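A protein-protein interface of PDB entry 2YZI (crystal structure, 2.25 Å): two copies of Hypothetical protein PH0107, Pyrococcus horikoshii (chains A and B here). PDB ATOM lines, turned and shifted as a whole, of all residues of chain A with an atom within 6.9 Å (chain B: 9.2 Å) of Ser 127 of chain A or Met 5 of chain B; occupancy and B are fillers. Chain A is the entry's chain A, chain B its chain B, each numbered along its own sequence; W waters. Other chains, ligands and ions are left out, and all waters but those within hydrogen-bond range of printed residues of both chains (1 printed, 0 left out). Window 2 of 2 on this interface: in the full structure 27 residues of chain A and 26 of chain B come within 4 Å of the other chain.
The side-chain hydroxyl (OG) of Ser 127 of chain A sits at hydrogen-bond distance from the backbone carbonyl oxygen (O) of Leu 123 of chain A (2.7 Å). The side-chain carboxylate (OE2) of Glu 125 of chain A lies within salt-bridge range of the guanidinium group (NH1) of Arg 128 of chain A, at 3.7 Å. The backbone carbonyl oxygen (O) of Met 5 of chain B lies within hydrogen-bond range of the backbone NH (N) of Gly 92 of chain B (3.0 Å). The backbone carbonyl oxygen of Leu 123 of chain B sits at hydrogen-bond distance from the side-chain hydroxyl of Ser 127 of chain B (3.3 Å). O of Leu 124 of chain B sits at hydrogen-bond distance from OG of Ser 127 of chain B, at 2.5 Å.
CD1 of Leu 120 of chain A touches O of Leu 120 of chain B, at 3.6 Å. Leu 124 of chain B touches Leu 120 of chain A. Leu 123 of chain B touches Leu 123 of chain A (CD2 to CG, 3.7 Å). Leu 124 of chain B touches Leu 123 of chain A (CA to CD2, 3.9 Å). Leu 95 of chain B touches Leu 124 of chain A (O to CD2, 3.95 Å). Leu 120 of chain B touches Leu 124 of chain A (CD2 to CD1, 3.7 Å). CD2 of Leu 123 of chain B touches CA of Leu 124 of chain A (3.5 Å). CE of Met 5 of chain B touches O of Ser 127 of chain A, at 3.4 Å. OG of Ser 127 of chain A touches CD1 of Leu 123 of chain B (3.9 Å). Arg 96 of chain B touches Arg 128 of chain A.
Of the printed residues of chain B, Leu 120 of chain A touches Leu 120 and Leu 124. No residue of chain B comes within 4 Å of Ala 126 of chain A. Of chain B, only Met 5 (3.4 Å), Leu 95 (3.7 Å) and Leu 123 (3.9 Å) come within 4 Å of Ser 127 of chain A. Met 5 of chain B touches just one residue of chain A: Ser 127 (3.4 Å). Of the printed residues of chain A, Arg 96 of chain B touches Arg 128 (3.4 Å). Printed residues of chain A within 4 Å of Leu 124 of chain B: Leu 120 (3.9 Å) and Leu 123 (3.9 Å). The nearest residue of chain A that does not touch Met 5 of chain B is Arg 128 of chain A (4.1 Å). The nearest printed residue of chain B that does not touch Leu 123 of chain A is Ser 127 of chain B (4.1 Å).
Of the 12 printed residues of chain A, 5 touch a printed residue of chain B. Hydrophobic or aromatic side chains of chain A within 4 Å of the printed part of chain B: Leu 120, Leu 123 and Leu 124. Among the printed residues, 11 pairs touch across the chains. Among the printed residues, no Asp or Glu carboxylate lies within 4 Å of a Lys or Arg side-chain nitrogen of the other chain.
Leu 120 of chain B touches its own counterpart, Leu 120 of chain A. Leu 123 of chain B touches its own counterpart, Leu 123 of chain A. Leu 123 of chain A touches Leu 124 of chain B, and with the chains exchanged Leu 124 of chain A touches Leu 123 of chain B. Ser 127 of chain A touches Leu 123 of chain B, but with the chains exchanged Leu 123 of chain A does not touch Ser 127 of chain B (4.1 Å).
Water W1 bridges NE of Arg 96 of chain B and NH2 of Arg 128 of chain A.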
ATOM      1  N   MET A   3      25.190   5.353  -3.122  1.00  0.00           N
ATOM      2  CA  MET A   3      23.871   4.683  -3.280  1.00  0.00           C
ATOM      3  C   MET A   3      23.525   4.628  -4.766  1.00  0.00           C
ATOM      4  O   MET A   3      24.022   5.427  -5.559  1.00  0.00           O
ATOM      5  CB  MET A   3      22.794   5.442  -2.491  1.00  0.00           C
ATOM      6  CG  MET A   3      22.396   6.800  -3.055  1.00  0.00           C
ATOM      7  SD  MET A   3      21.526   7.981  -1.736  1.00  0.00           S
ATOM      8  CE  MET A   3      22.334   9.654  -2.297  1.00  0.00           C
ATOM      9  N   TYR A  12      16.010   0.745   0.420  1.00  0.00           N
ATOM     10  CA  TYR A  12      16.325   1.849   1.327  1.00  0.00           C
ATOM     11  C   TYR A  12      15.206   2.325   2.246  1.00  0.00           C
ATOM     12  O   TYR A  12      15.453   3.117   3.153  1.00  0.00           O
ATOM     13  CB  TYR A  12      16.791   3.065   0.514  1.00  0.00           C
ATOM     14  CG  TYR A  12      17.984   2.839  -0.387  1.00  0.00           C
ATOM     15  CD1 TYR A  12      19.213   2.438   0.131  1.00  0.00           C
ATOM     16  CD2 TYR A  12      17.891   3.063  -1.753  1.00  0.00           C
ATOM     17  CE1 TYR A  12      20.318   2.274  -0.690  1.00  0.00           C
ATOM     18  CE2 TYR A  12      18.986   2.899  -2.582  1.00  0.00           C
ATOM     19  CZ  TYR A  12      20.200   2.507  -2.044  1.00  0.00           C
ATOM     20  OH  TYR A  12      21.298   2.380  -2.867  1.00  0.00           O
ATOM     21  N   LEU A 120      13.095  11.656   3.787  1.00  0.00           N
ATOM     22  CA  LEU A 120      14.402  12.221   3.524  1.00  0.00           C
ATOM     23  C   LEU A 120      15.370  11.744   4.592  1.00  0.00           C
ATOM     24  O   LEU A 120      16.581  11.786   4.387  1.00  0.00           O
ATOM     25  CB  LEU A 120      14.346  13.744   3.507  1.00  0.00           C
ATOM     26  CG  LEU A 120      13.565  14.384   2.357  1.00  0.00           C
ATOM     27  CD1 LEU A 120      13.670  15.896   2.494  1.00  0.00           C
ATOM     28  CD2 LEU A 120      14.106  13.935   0.998  1.00  0.00           C
ATOM     29  N   ASP A 122      15.426   8.686   5.578  1.00  0.00           N
ATOM     30  CA  ASP A 122      15.861   7.411   5.022  1.00  0.00           C
ATOM     31  C   ASP A 122      16.868   7.719   3.931  1.00  0.00           C
ATOM     32  O   ASP A 122      17.796   6.936   3.690  1.00  0.00           O
ATOM     33  CB  ASP A 122      14.689   6.635   4.434  1.00  0.00           C
ATOM     34  CG  ASP A 122      13.750   6.115   5.495  1.00  0.00           C
ATOM     35  OD1 ASP A 122      14.238   5.451   6.436  1.00  0.00           O
ATOM     36  OD2 ASP A 122      12.526   6.364   5.387  1.00  0.00           O
ATOM     37  N   LEU A 123      16.687   8.867   3.278  1.00  0.00           N
ATOM     38  CA  LEU A 123      17.610   9.288   2.222  1.00  0.00           C
ATOM     39  C   LEU A 123      18.995   9.504   2.833  1.00  0.00           C
ATOM     40  O   LEU A 123      20.004   9.066   2.274  1.00  0.00           O
ATOM     41  CB  LEU A 123      17.135  10.580   1.551  1.00  0.00           C
ATOM     42  CG  LEU A 123      18.101  11.227   0.542  1.00  0.00           C
ATOM     43  CD1 LEU A 123      18.439  10.253  -0.581  1.00  0.00           C
ATOM     44  CD2 LEU A 123      17.467  12.491  -0.030  1.00  0.00           C
ATOM     45  N   LEU A 124      19.030  10.158   3.992  1.00  0.00           N
ATOM     46  CA  LEU A 124      20.287  10.429   4.676  1.00  0.00           C
ATOM     47  C   LEU A 124      21.015   9.125   4.997  1.00  0.00           C
ATOM     48  O   LEU A 124      22.216   9.002   4.744  1.00  0.00           O
ATOM     49  CB  LEU A 124      20.036  11.237   5.958  1.00  0.00           C
ATOM     50  CG  LEU A 124      21.283  11.647   6.757  1.00  0.00           C
ATOM     51  CD1 LEU A 124      20.991  12.884   7.575  1.00  0.00           C
ATOM     52  CD2 LEU A 124      21.729  10.505   7.656  1.00  0.00           C
ATOM     53  N   GLU A 125      20.294   8.157   5.556  1.00  0.00           N
ATOM     54  CA  GLU A 125      20.898   6.871   5.876  1.00  0.00           C
ATOM     55  C   GLU A 125      21.408   6.154   4.622  1.00  0.00           C
ATOM     56  O   GLU A 125      22.504   5.599   4.630  1.00  0.00           O
ATOM     57  CB  GLU A 125      19.907   5.984   6.632  1.00  0.00           C
ATOM     58  CG  GLU A 125      19.857   6.282   8.124  1.00  0.00           C
ATOM     59  CD  GLU A 125      21.243   6.219   8.763  1.00  0.00           C
ATOM     60  OE1 GLU A 125      21.921   5.181   8.596  1.00  0.00           O
ATOM     61  OE2 GLU A 125      21.656   7.198   9.425  1.00  0.00           O
ATOM     62  N   ALA A 126      20.624   6.181   3.544  1.00  0.00           N
ATOM     63  CA  ALA A 126      21.042   5.548   2.297  1.00  0.00           C
ATOM     64  C   ALA A 126      22.304   6.237   1.790  1.00  0.00           C
ATOM     65  O   ALA A 126      23.195   5.601   1.236  1.00  0.00           O
ATOM     66  CB  ALA A 126      19.945   5.658   1.253  1.00  0.00           C
ATOM     67  N   SER A 127      22.367   7.547   1.984  1.00  0.00           N
ATOM     68  CA  SER A 127      23.519   8.330   1.559  1.00  0.00           C
ATOM     69  C   SER A 127      24.796   7.849   2.238  1.00  0.00           C
ATOM     70  O   SER A 127      25.871   7.887   1.647  1.00  0.00           O
ATOM     71  CB  SER A 127      23.310   9.810   1.895  1.00  0.00           C
ATOM     72  OG  SER A 127      22.180  10.324   1.221  1.00  0.00           O
ATOM     73  N   ARG A 128      24.669   7.400   3.482  1.00  0.00           N
ATOM     74  CA  ARG A 128      25.824   6.942   4.242  1.00  0.00           C
ATOM     75  C   ARG A 128      26.163   5.471   4.054  1.00  0.00           C
ATOM     76  O   ARG A 128      27.241   5.038   4.454  1.00  0.00           O
ATOM     77  CB  ARG A 128      25.624   7.209   5.738  1.00  0.00           C
ATOM     78  CG  ARG A 128      25.356   8.656   6.111  1.00  0.00           C
ATOM     79  CD  ARG A 128      25.179   8.792   7.620  1.00  0.00           C
ATOM     80  NE  ARG A 128      26.405   8.454   8.340  1.00  0.00           N
ATOM     81  CZ  ARG A 128      26.445   7.731   9.456  1.00  0.00           C
ATOM     82  NH1 ARG A 128      25.323   7.259   9.986  1.00  0.00           N
ATOM     83  NH2 ARG A 128      27.606   7.501  10.053  1.00  0.00           N
ATOM     84  N   ARG A 129      25.269   4.690   3.461  1.00  0.00           N
ATOM     85  CA  ARG A 129      25.588   3.282   3.299  1.00  0.00           C
ATOM     86  C   ARG A 129      26.835   3.088   2.442  1.00  0.00           C
ATOM     87  O   ARG A 129      27.034   3.787   1.450  1.00  0.00           O
ATOM     88  CB  ARG A 129      24.378   2.520   2.752  1.00  0.00           C
ATOM     89  CG  ARG A 129      23.536   1.960   3.896  1.00  0.00           C
ATOM     90  CD  ARG A 129      22.092   1.675   3.538  1.00  0.00           C
ATOM     91  NE  ARG A 129      21.938   0.565   2.610  1.00  0.00           N
ATOM     92  CZ  ARG A 129      20.793  -0.084   2.431  1.00  0.00           C
ATOM     93  NH1 ARG A 129      19.721   0.274   3.125  1.00  0.00           N
ATOM     94  NH2 ARG A 129      20.720  -1.087   1.565  1.00  0.00           N
ATOM     95  N   ARG A 130      27.686   2.154   2.858  1.00  0.00           N
ATOM     96  CA  ARG A 130      28.946   1.875   2.178  1.00  0.00           C
ATOM     97  C   ARG A 130      28.881   0.749   1.156  1.00  0.00           C
ATOM     98  O   ARG A 130      29.700   0.694   0.246  1.00  0.00           O
ATOM     99  CB  ARG A 130      30.023   1.558   3.214  1.00  0.00           C
ATOM    100  CG  ARG A 130      30.164   2.626   4.279  1.00  0.00           C
ATOM    101  CD  ARG A 130      30.594   3.947   3.660  1.00  0.00           C
ATOM    102  NE  ARG A 130      31.968   3.887   3.172  1.00  0.00           N
ATOM    103  CZ  ARG A 130      33.036   3.924   3.962  1.00  0.00           C
ATOM    104  NH1 ARG A 130      32.881   4.024   5.276  1.00  0.00           N
ATOM    105  NH2 ARG A 130      34.255   3.855   3.439  1.00  0.00           N
ATOM    106  N   MET B   3      26.566  14.844  -5.796  1.00  0.00           N
ATOM    107  CA  MET B   3      27.120  15.170  -4.450  1.00  0.00           C
ATOM    108  C   MET B   3      28.346  14.328  -4.108  1.00  0.00           C
ATOM    109  O   MET B   3      28.433  13.149  -4.455  1.00  0.00           O
ATOM    110  CB  MET B   3      26.047  14.991  -3.369  1.00  0.00           C
ATOM    111  CG  MET B   3      25.358  13.646  -3.386  1.00  0.00           C
ATOM    112  SD  MET B   3      24.158  13.430  -1.875  1.00  0.00           S
ATOM    113  CE  MET B   3      25.184  12.162  -0.828  1.00  0.00           C
ATOM    114  N   ASP B   4      29.282  14.960  -3.410  1.00  0.00           N
ATOM    115  CA  ASP B   4      30.533  14.341  -3.010  1.00  0.00           C
ATOM    116  C   ASP B   4      30.710  14.415  -1.496  1.00  0.00           C
ATOM    117  O   ASP B   4      30.875  15.492  -0.939  1.00  0.00           O
ATOM    118  CB  ASP B   4      31.684  15.059  -3.731  1.00  0.00           C
ATOM    119  CG  ASP B   4      33.049  14.610  -3.260  1.00  0.00           C
ATOM    120  OD1 ASP B   4      33.150  13.502  -2.700  1.00  0.00           O
ATOM    121  OD2 ASP B   4      34.021  15.368  -3.469  1.00  0.00           O
ATOM    122  N   MET B   5      30.678  13.256  -0.846  1.00  0.00           N
ATOM    123  CA  MET B   5      30.827  13.150   0.604  1.00  0.00           C
ATOM    124  C   MET B   5      32.126  13.767   1.112  1.00  0.00           C
ATOM    125  O   MET B   5      32.260  14.054   2.302  1.00  0.00           O
ATOM    126  CB  MET B   5      30.779  11.684   1.022  1.00  0.00           C
ATOM    127  CG  MET B   5      29.521  10.964   0.596  1.00  0.00           C
ATOM    128  SD  MET B   5      27.994  11.510   1.650  1.00  0.00           S
ATOM    129  CE  MET B   5      28.104  10.094   2.982  1.00  0.00           C
ATOM    130  N   LYS B   6      33.079  13.968   0.209  1.00  0.00           N
ATOM    131  CA  LYS B   6      34.369  14.538   0.573  1.00  0.00           C
ATOM    132  C   LYS B   6      34.357  16.061   0.575  1.00  0.00           C
ATOM    133  O   LYS B   6      35.120  16.684   1.310  1.00  0.00           O
ATOM    134  CB  LYS B   6      35.455  14.046  -0.389  1.00  0.00           C
ATOM    135  CG  LYS B   6      35.656  12.537  -0.383  1.00  0.00           C
ATOM    136  CD  LYS B   6      36.562  12.093  -1.529  1.00  0.00           C
ATOM    137  CE  LYS B   6      36.638  10.574  -1.650  1.00  0.00           C
ATOM    138  NZ  LYS B   6      37.226   9.914  -0.442  1.00  0.00           N
ATOM    139  N   ALA B   7      33.492  16.652  -0.243  1.00  0.00           N
ATOM    140  CA  ALA B   7      33.394  18.108  -0.360  1.00  0.00           C
ATOM    141  C   ALA B   7      32.887  18.818   0.895  1.00  0.00           C
ATOM    142  O   ALA B   7      32.079  18.278   1.640  1.00  0.00           O
ATOM    143  CB  ALA B   7      32.509  18.462  -1.545  1.00  0.00           C
ATOM    144  N   PRO B   8      33.346  20.056   1.127  1.00  0.00           N
ATOM    145  CA  PRO B   8      32.946  20.856   2.293  1.00  0.00           C
ATOM    146  C   PRO B   8      31.455  21.143   2.275  1.00  0.00           C
ATOM    147  O   PRO B   8      30.883  21.401   1.210  1.00  0.00           O
ATOM    148  CB  PRO B   8      33.767  22.125   2.131  1.00  0.00           C
ATOM    149  CG  PRO B   8      33.811  22.277   0.652  1.00  0.00           C
ATOM    150  CD  PRO B   8      34.141  20.871   0.196  1.00  0.00           C
ATOM    151  N   ILE B   9      30.833  21.118   3.453  1.00  0.00           N
ATOM    152  CA  ILE B   9      29.397  21.351   3.561  1.00  0.00           C
ATOM    153  C   ILE B   9      28.986  22.704   3.002  1.00  0.00           C
ATOM    154  O   ILE B   9      27.834  22.908   2.638  1.00  0.00           O
ATOM    155  CB  ILE B   9      28.899  21.255   5.035  1.00  0.00           C
ATOM    156  CG1 ILE B   9      27.386  21.016   5.051  1.00  0.00           C
ATOM    157  CG2 ILE B   9      29.198  22.548   5.800  1.00  0.00           C
ATOM    158  CD1 ILE B   9      26.976  19.696   4.447  1.00  0.00           C
ATOM    159  N   VAL B  11      29.227  23.875   0.251  1.00  0.00           N
ATOM    160  CA  VAL B  11      28.719  23.853  -1.116  1.00  0.00           C
ATOM    161  C   VAL B  11      27.269  23.372  -1.207  1.00  0.00           C
ATOM    162  O   VAL B  11      26.581  23.627  -2.197  1.00  0.00           O
ATOM    163  CB  VAL B  11      29.603  22.979  -2.048  1.00  0.00           C
ATOM    164  CG1 VAL B  11      31.061  23.191  -1.714  1.00  0.00           C
ATOM    165  CG2 VAL B  11      29.219  21.520  -1.947  1.00  0.00           C
ATOM    166  N   TYR B  12      26.799  22.688  -0.172  1.00  0.00           N
ATOM    167  CA  TYR B  12      25.431  22.184  -0.173  1.00  0.00           C
ATOM    168  C   TYR B  12      24.515  22.966   0.771  1.00  0.00           C
ATOM    169  O   TYR B  12      23.297  22.792   0.745  1.00  0.00           O
ATOM    170  CB  TYR B  12      25.425  20.710   0.221  1.00  0.00           C
ATOM    171  CG  TYR B  12      26.388  19.860  -0.566  1.00  0.00           C
ATOM    172  CD1 TYR B  12      26.176  19.597  -1.917  1.00  0.00           C
ATOM    173  CD2 TYR B  12      27.512  19.306   0.044  1.00  0.00           C
ATOM    174  CE1 TYR B  12      27.062  18.796  -2.642  1.00  0.00           C
ATOM    175  CE2 TYR B  12      28.407  18.505  -0.667  1.00  0.00           C
ATOM    176  CZ  TYR B  12      28.171  18.255  -2.009  1.00  0.00           C
ATOM    177  OH  TYR B  12      29.042  17.458  -2.712  1.00  0.00           O
ATOM    178  N   ASN B  88      33.774  24.111   6.420  1.00  0.00           N
ATOM    179  CA  ASN B  88      34.725  23.202   5.789  1.00  0.00           C
ATOM    180  C   ASN B  88      34.556  21.723   6.118  1.00  0.00           C
ATOM    181  O   ASN B  88      35.238  20.887   5.537  1.00  0.00           O
ATOM    182  CB  ASN B  88      36.154  23.638   6.112  1.00  0.00           C
ATOM    183  CG  ASN B  88      36.534  24.921   5.413  1.00  0.00           C
ATOM    184  OD1 ASN B  88      37.300  25.722   5.943  1.00  0.00           O
ATOM    185  ND2 ASN B  88      36.010  25.121   4.213  1.00  0.00           N
ATOM    186  N   THR B  89      33.659  21.405   7.048  1.00  0.00           N
ATOM    187  CA  THR B  89      33.390  20.019   7.418  1.00  0.00           C
ATOM    188  C   THR B  89      32.812  19.332   6.185  1.00  0.00           C
ATOM    189  O   THR B  89      31.839  19.809   5.617  1.00  0.00           O
ATOM    190  CB  THR B  89      32.322  19.923   8.545  1.00  0.00           C
ATOM    191  OG1 THR B  89      32.745  20.667   9.693  1.00  0.00           O
ATOM    192  CG2 THR B  89      32.087  18.469   8.937  1.00  0.00           C
ATOM    193  N   PRO B  90      33.406  18.207   5.753  1.00  0.00           N
ATOM    194  CA  PRO B  90      32.912  17.483   4.578  1.00  0.00           C
ATOM    195  C   PRO B  90      31.514  16.897   4.778  1.00  0.00           C
ATOM    196  O   PRO B  90      31.164  16.424   5.867  1.00  0.00           O
ATOM    197  CB  PRO B  90      33.967  16.399   4.371  1.00  0.00           C
ATOM    198  CG  PRO B  90      34.437  16.131   5.762  1.00  0.00           C
ATOM    199  CD  PRO B  90      34.587  17.534   6.314  1.00  0.00           C
ATOM    200  N   LEU B  91      30.725  16.940   3.712  1.00  0.00           N
ATOM    201  CA  LEU B  91      29.360  16.438   3.713  1.00  0.00           C
ATOM    202  C   LEU B  91      29.148  15.163   4.530  1.00  0.00           C
ATOM    203  O   LEU B  91      28.280  15.125   5.405  1.00  0.00           O
ATOM    204  CB  LEU B  91      28.903  16.194   2.274  1.00  0.00           C
ATOM    205  CG  LEU B  91      27.502  15.612   2.101  1.00  0.00           C
ATOM    206  CD1 LEU B  91      26.495  16.547   2.730  1.00  0.00           C
ATOM    207  CD2 LEU B  91      27.190  15.397   0.626  1.00  0.00           C
ATOM    208  N   GLY B  92      29.932  14.128   4.234  1.00  0.00           N
ATOM    209  CA  GLY B  92      29.813  12.860   4.937  1.00  0.00           C
ATOM    210  C   GLY B  92      29.797  12.974   6.448  1.00  0.00           C
ATOM    211  O   GLY B  92      28.920  12.412   7.104  1.00  0.00           O
ATOM    212  N   GLU B  93      30.771  13.695   6.996  1.00  0.00           N
ATOM    213  CA  GLU B  93      30.876  13.899   8.436  1.00  0.00           C
ATOM    214  C   GLU B  93      29.682  14.687   8.981  1.00  0.00           C
ATOM    215  O   GLU B  93      29.242  14.470  10.121  1.00  0.00           O
ATOM    216  CB  GLU B  93      32.180  14.630   8.770  1.00  0.00           C
ATOM    217  CG  GLU B  93      33.437  13.826   8.451  1.00  0.00           C
ATOM    218  CD  GLU B  93      34.723  14.579   8.780  1.00  0.00           C
ATOM    219  OE1 GLU B  93      34.808  15.162   9.884  1.00  0.00           O
ATOM    220  OE2 GLU B  93      35.654  14.580   7.945  1.00  0.00           O
ATOM    221  N   VAL B  94      29.157  15.604   8.174  1.00  0.00           N
ATOM    222  CA  VAL B  94      28.005  16.391   8.594  1.00  0.00           C
ATOM    223  C   VAL B  94      26.797  15.465   8.688  1.00  0.00           C
ATOM    224  O   VAL B  94      26.037  15.511   9.655  1.00  0.00           O
ATOM    225  CB  VAL B  94      27.727  17.537   7.602  1.00  0.00           C
ATOM    226  CG1 VAL B  94      26.369  18.187   7.904  1.00  0.00           C
ATOM    227  CG2 VAL B  94      28.840  18.574   7.712  1.00  0.00           C
ATOM    228  N   LEU B  95      26.634  14.608   7.683  1.00  0.00           N
ATOM    229  CA  LEU B  95      25.533  13.646   7.667  1.00  0.00           C
ATOM    230  C   LEU B  95      25.606  12.731   8.889  1.00  0.00           C
ATOM    231  O   LEU B  95      24.596  12.462   9.546  1.00  0.00           O
ATOM    232  CB  LEU B  95      25.587  12.801   6.398  1.00  0.00           C
ATOM    233  CG  LEU B  95      24.690  13.222   5.235  1.00  0.00           C
ATOM    234  CD1 LEU B  95      24.871  14.687   4.938  1.00  0.00           C
ATOM    235  CD2 LEU B  95      25.014  12.370   4.012  1.00  0.00           C
ATOM    236  N   ARG B  96      26.804  12.252   9.189  1.00  0.00           N
ATOM    237  CA  ARG B  96      26.992  11.383  10.333  1.00  0.00           C
ATOM    238  C   ARG B  96      26.614  12.118  11.628  1.00  0.00           C
ATOM    239  O   ARG B  96      25.967  11.560  12.518  1.00  0.00           O
ATOM    240  CB  ARG B  96      28.442  10.914  10.398  1.00  0.00           C
ATOM    241  CG  ARG B  96      28.786  10.198  11.693  1.00  0.00           C
ATOM    242  CD  ARG B  96      30.203   9.661  11.693  1.00  0.00           C
ATOM    243  NE  ARG B  96      30.453   8.846  12.873  1.00  0.00           N
ATOM    244  CZ  ARG B  96      31.565   8.149  13.081  1.00  0.00           C
ATOM    245  NH1 ARG B  96      32.539   8.165  12.185  1.00  0.00           N
ATOM    246  NH2 ARG B  96      31.696   7.431  14.183  1.00  0.00           N
ATOM    247  N   PHE B 118      22.116  23.577   6.903  1.00  0.00           N
ATOM    248  CA  PHE B 118      22.006  22.452   5.990  1.00  0.00           C
ATOM    249  C   PHE B 118      20.832  21.607   6.467  1.00  0.00           C
ATOM    250  O   PHE B 118      20.767  21.226   7.635  1.00  0.00           O
ATOM    251  CB  PHE B 118      23.283  21.613   5.980  1.00  0.00           C
ATOM    252  CG  PHE B 118      23.197  20.396   5.089  1.00  0.00           C
ATOM    253  CD1 PHE B 118      23.100  20.533   3.707  1.00  0.00           C
ATOM    254  CD2 PHE B 118      23.190  19.121   5.636  1.00  0.00           C
ATOM    255  CE1 PHE B 118      22.993  19.411   2.871  1.00  0.00           C
ATOM    256  CE2 PHE B 118      23.084  17.981   4.807  1.00  0.00           C
ATOM    257  CZ  PHE B 118      22.985  18.133   3.422  1.00  0.00           C
ATOM    258  N   LEU B 120      17.595  18.457   5.392  1.00  0.00           N
ATOM    259  CA  LEU B 120      17.391  17.233   4.630  1.00  0.00           C
ATOM    260  C   LEU B 120      16.919  17.602   3.235  1.00  0.00           C
ATOM    261  O   LEU B 120      17.169  16.874   2.276  1.00  0.00           O
ATOM    262  CB  LEU B 120      16.379  16.311   5.314  1.00  0.00           C
ATOM    263  CG  LEU B 120      16.874  15.672   6.619  1.00  0.00           C
ATOM    264  CD1 LEU B 120      16.024  14.456   6.935  1.00  0.00           C
ATOM    265  CD2 LEU B 120      18.333  15.258   6.485  1.00  0.00           C
ATOM    266  N   ASP B 122      18.031  20.096   1.591  1.00  0.00           N
ATOM    267  CA  ASP B 122      19.259  20.409   0.872  1.00  0.00           C
ATOM    268  C   ASP B 122      19.886  19.111   0.358  1.00  0.00           C
ATOM    269  O   ASP B 122      20.394  19.060  -0.764  1.00  0.00           O
ATOM    270  CB  ASP B 122      20.246  21.139   1.778  1.00  0.00           C
ATOM    271  CG  ASP B 122      19.784  22.533   2.136  1.00  0.00           C
ATOM    272  OD1 ASP B 122      19.574  23.347   1.212  1.00  0.00           O
ATOM    273  OD2 ASP B 122      19.637  22.821   3.343  1.00  0.00           O
ATOM    274  N   LEU B 123      19.837  18.066   1.184  1.00  0.00           N
ATOM    275  CA  LEU B 123      20.375  16.762   0.820  1.00  0.00           C
ATOM    276  C   LEU B 123      19.683  16.272  -0.444  1.00  0.00           C
ATOM    277  O   LEU B 123      20.325  15.765  -1.365  1.00  0.00           O
ATOM    278  CB  LEU B 123      20.134  15.755   1.940  1.00  0.00           C
ATOM    279  CG  LEU B 123      20.548  14.312   1.629  1.00  0.00           C
ATOM    280  CD1 LEU B 123      22.054  14.264   1.391  1.00  0.00           C
ATOM    281  CD2 LEU B 123      20.147  13.384   2.783  1.00  0.00           C
ATOM    282  N   LEU B 124      18.363  16.414  -0.467  1.00  0.00           N
ATOM    283  CA  LEU B 124      17.567  16.014  -1.611  1.00  0.00           C
ATOM    284  C   LEU B 124      18.033  16.788  -2.838  1.00  0.00           C
ATOM    285  O   LEU B 124      18.171  16.228  -3.933  1.00  0.00           O
ATOM    286  CB  LEU B 124      16.088  16.306  -1.358  1.00  0.00           C
ATOM    287  CG  LEU B 124      15.188  15.903  -2.529  1.00  0.00           C
ATOM    288  CD1 LEU B 124      15.339  14.388  -2.758  1.00  0.00           C
ATOM    289  CD2 LEU B 124      13.729  16.285  -2.255  1.00  0.00           C
ATOM    290  N   ALA B 126      20.997  18.121  -3.377  1.00  0.00           N
ATOM    291  CA  ALA B 126      22.306  17.633  -3.783  1.00  0.00           C
ATOM    292  C   ALA B 126      22.192  16.275  -4.481  1.00  0.00           C
ATOM    293  O   ALA B 126      22.873  16.028  -5.473  1.00  0.00           O
ATOM    294  CB  ALA B 126      23.220  17.530  -2.574  1.00  0.00           C
ATOM    295  N   SER B 127      21.326  15.403  -3.971  1.00  0.00           N
ATOM    296  CA  SER B 127      21.138  14.085  -4.568  1.00  0.00           C
ATOM    297  C   SER B 127      20.583  14.189  -5.984  1.00  0.00           C
ATOM    298  O   SER B 127      20.716  13.262  -6.775  1.00  0.00           O
ATOM    299  CB  SER B 127      20.187  13.246  -3.719  1.00  0.00           C
ATOM    300  OG  SER B 127      18.902  13.828  -3.683  1.00  0.00           O
HETATM  301  O   HOH W   1      28.294   6.475  13.037  1.00  0.00           O
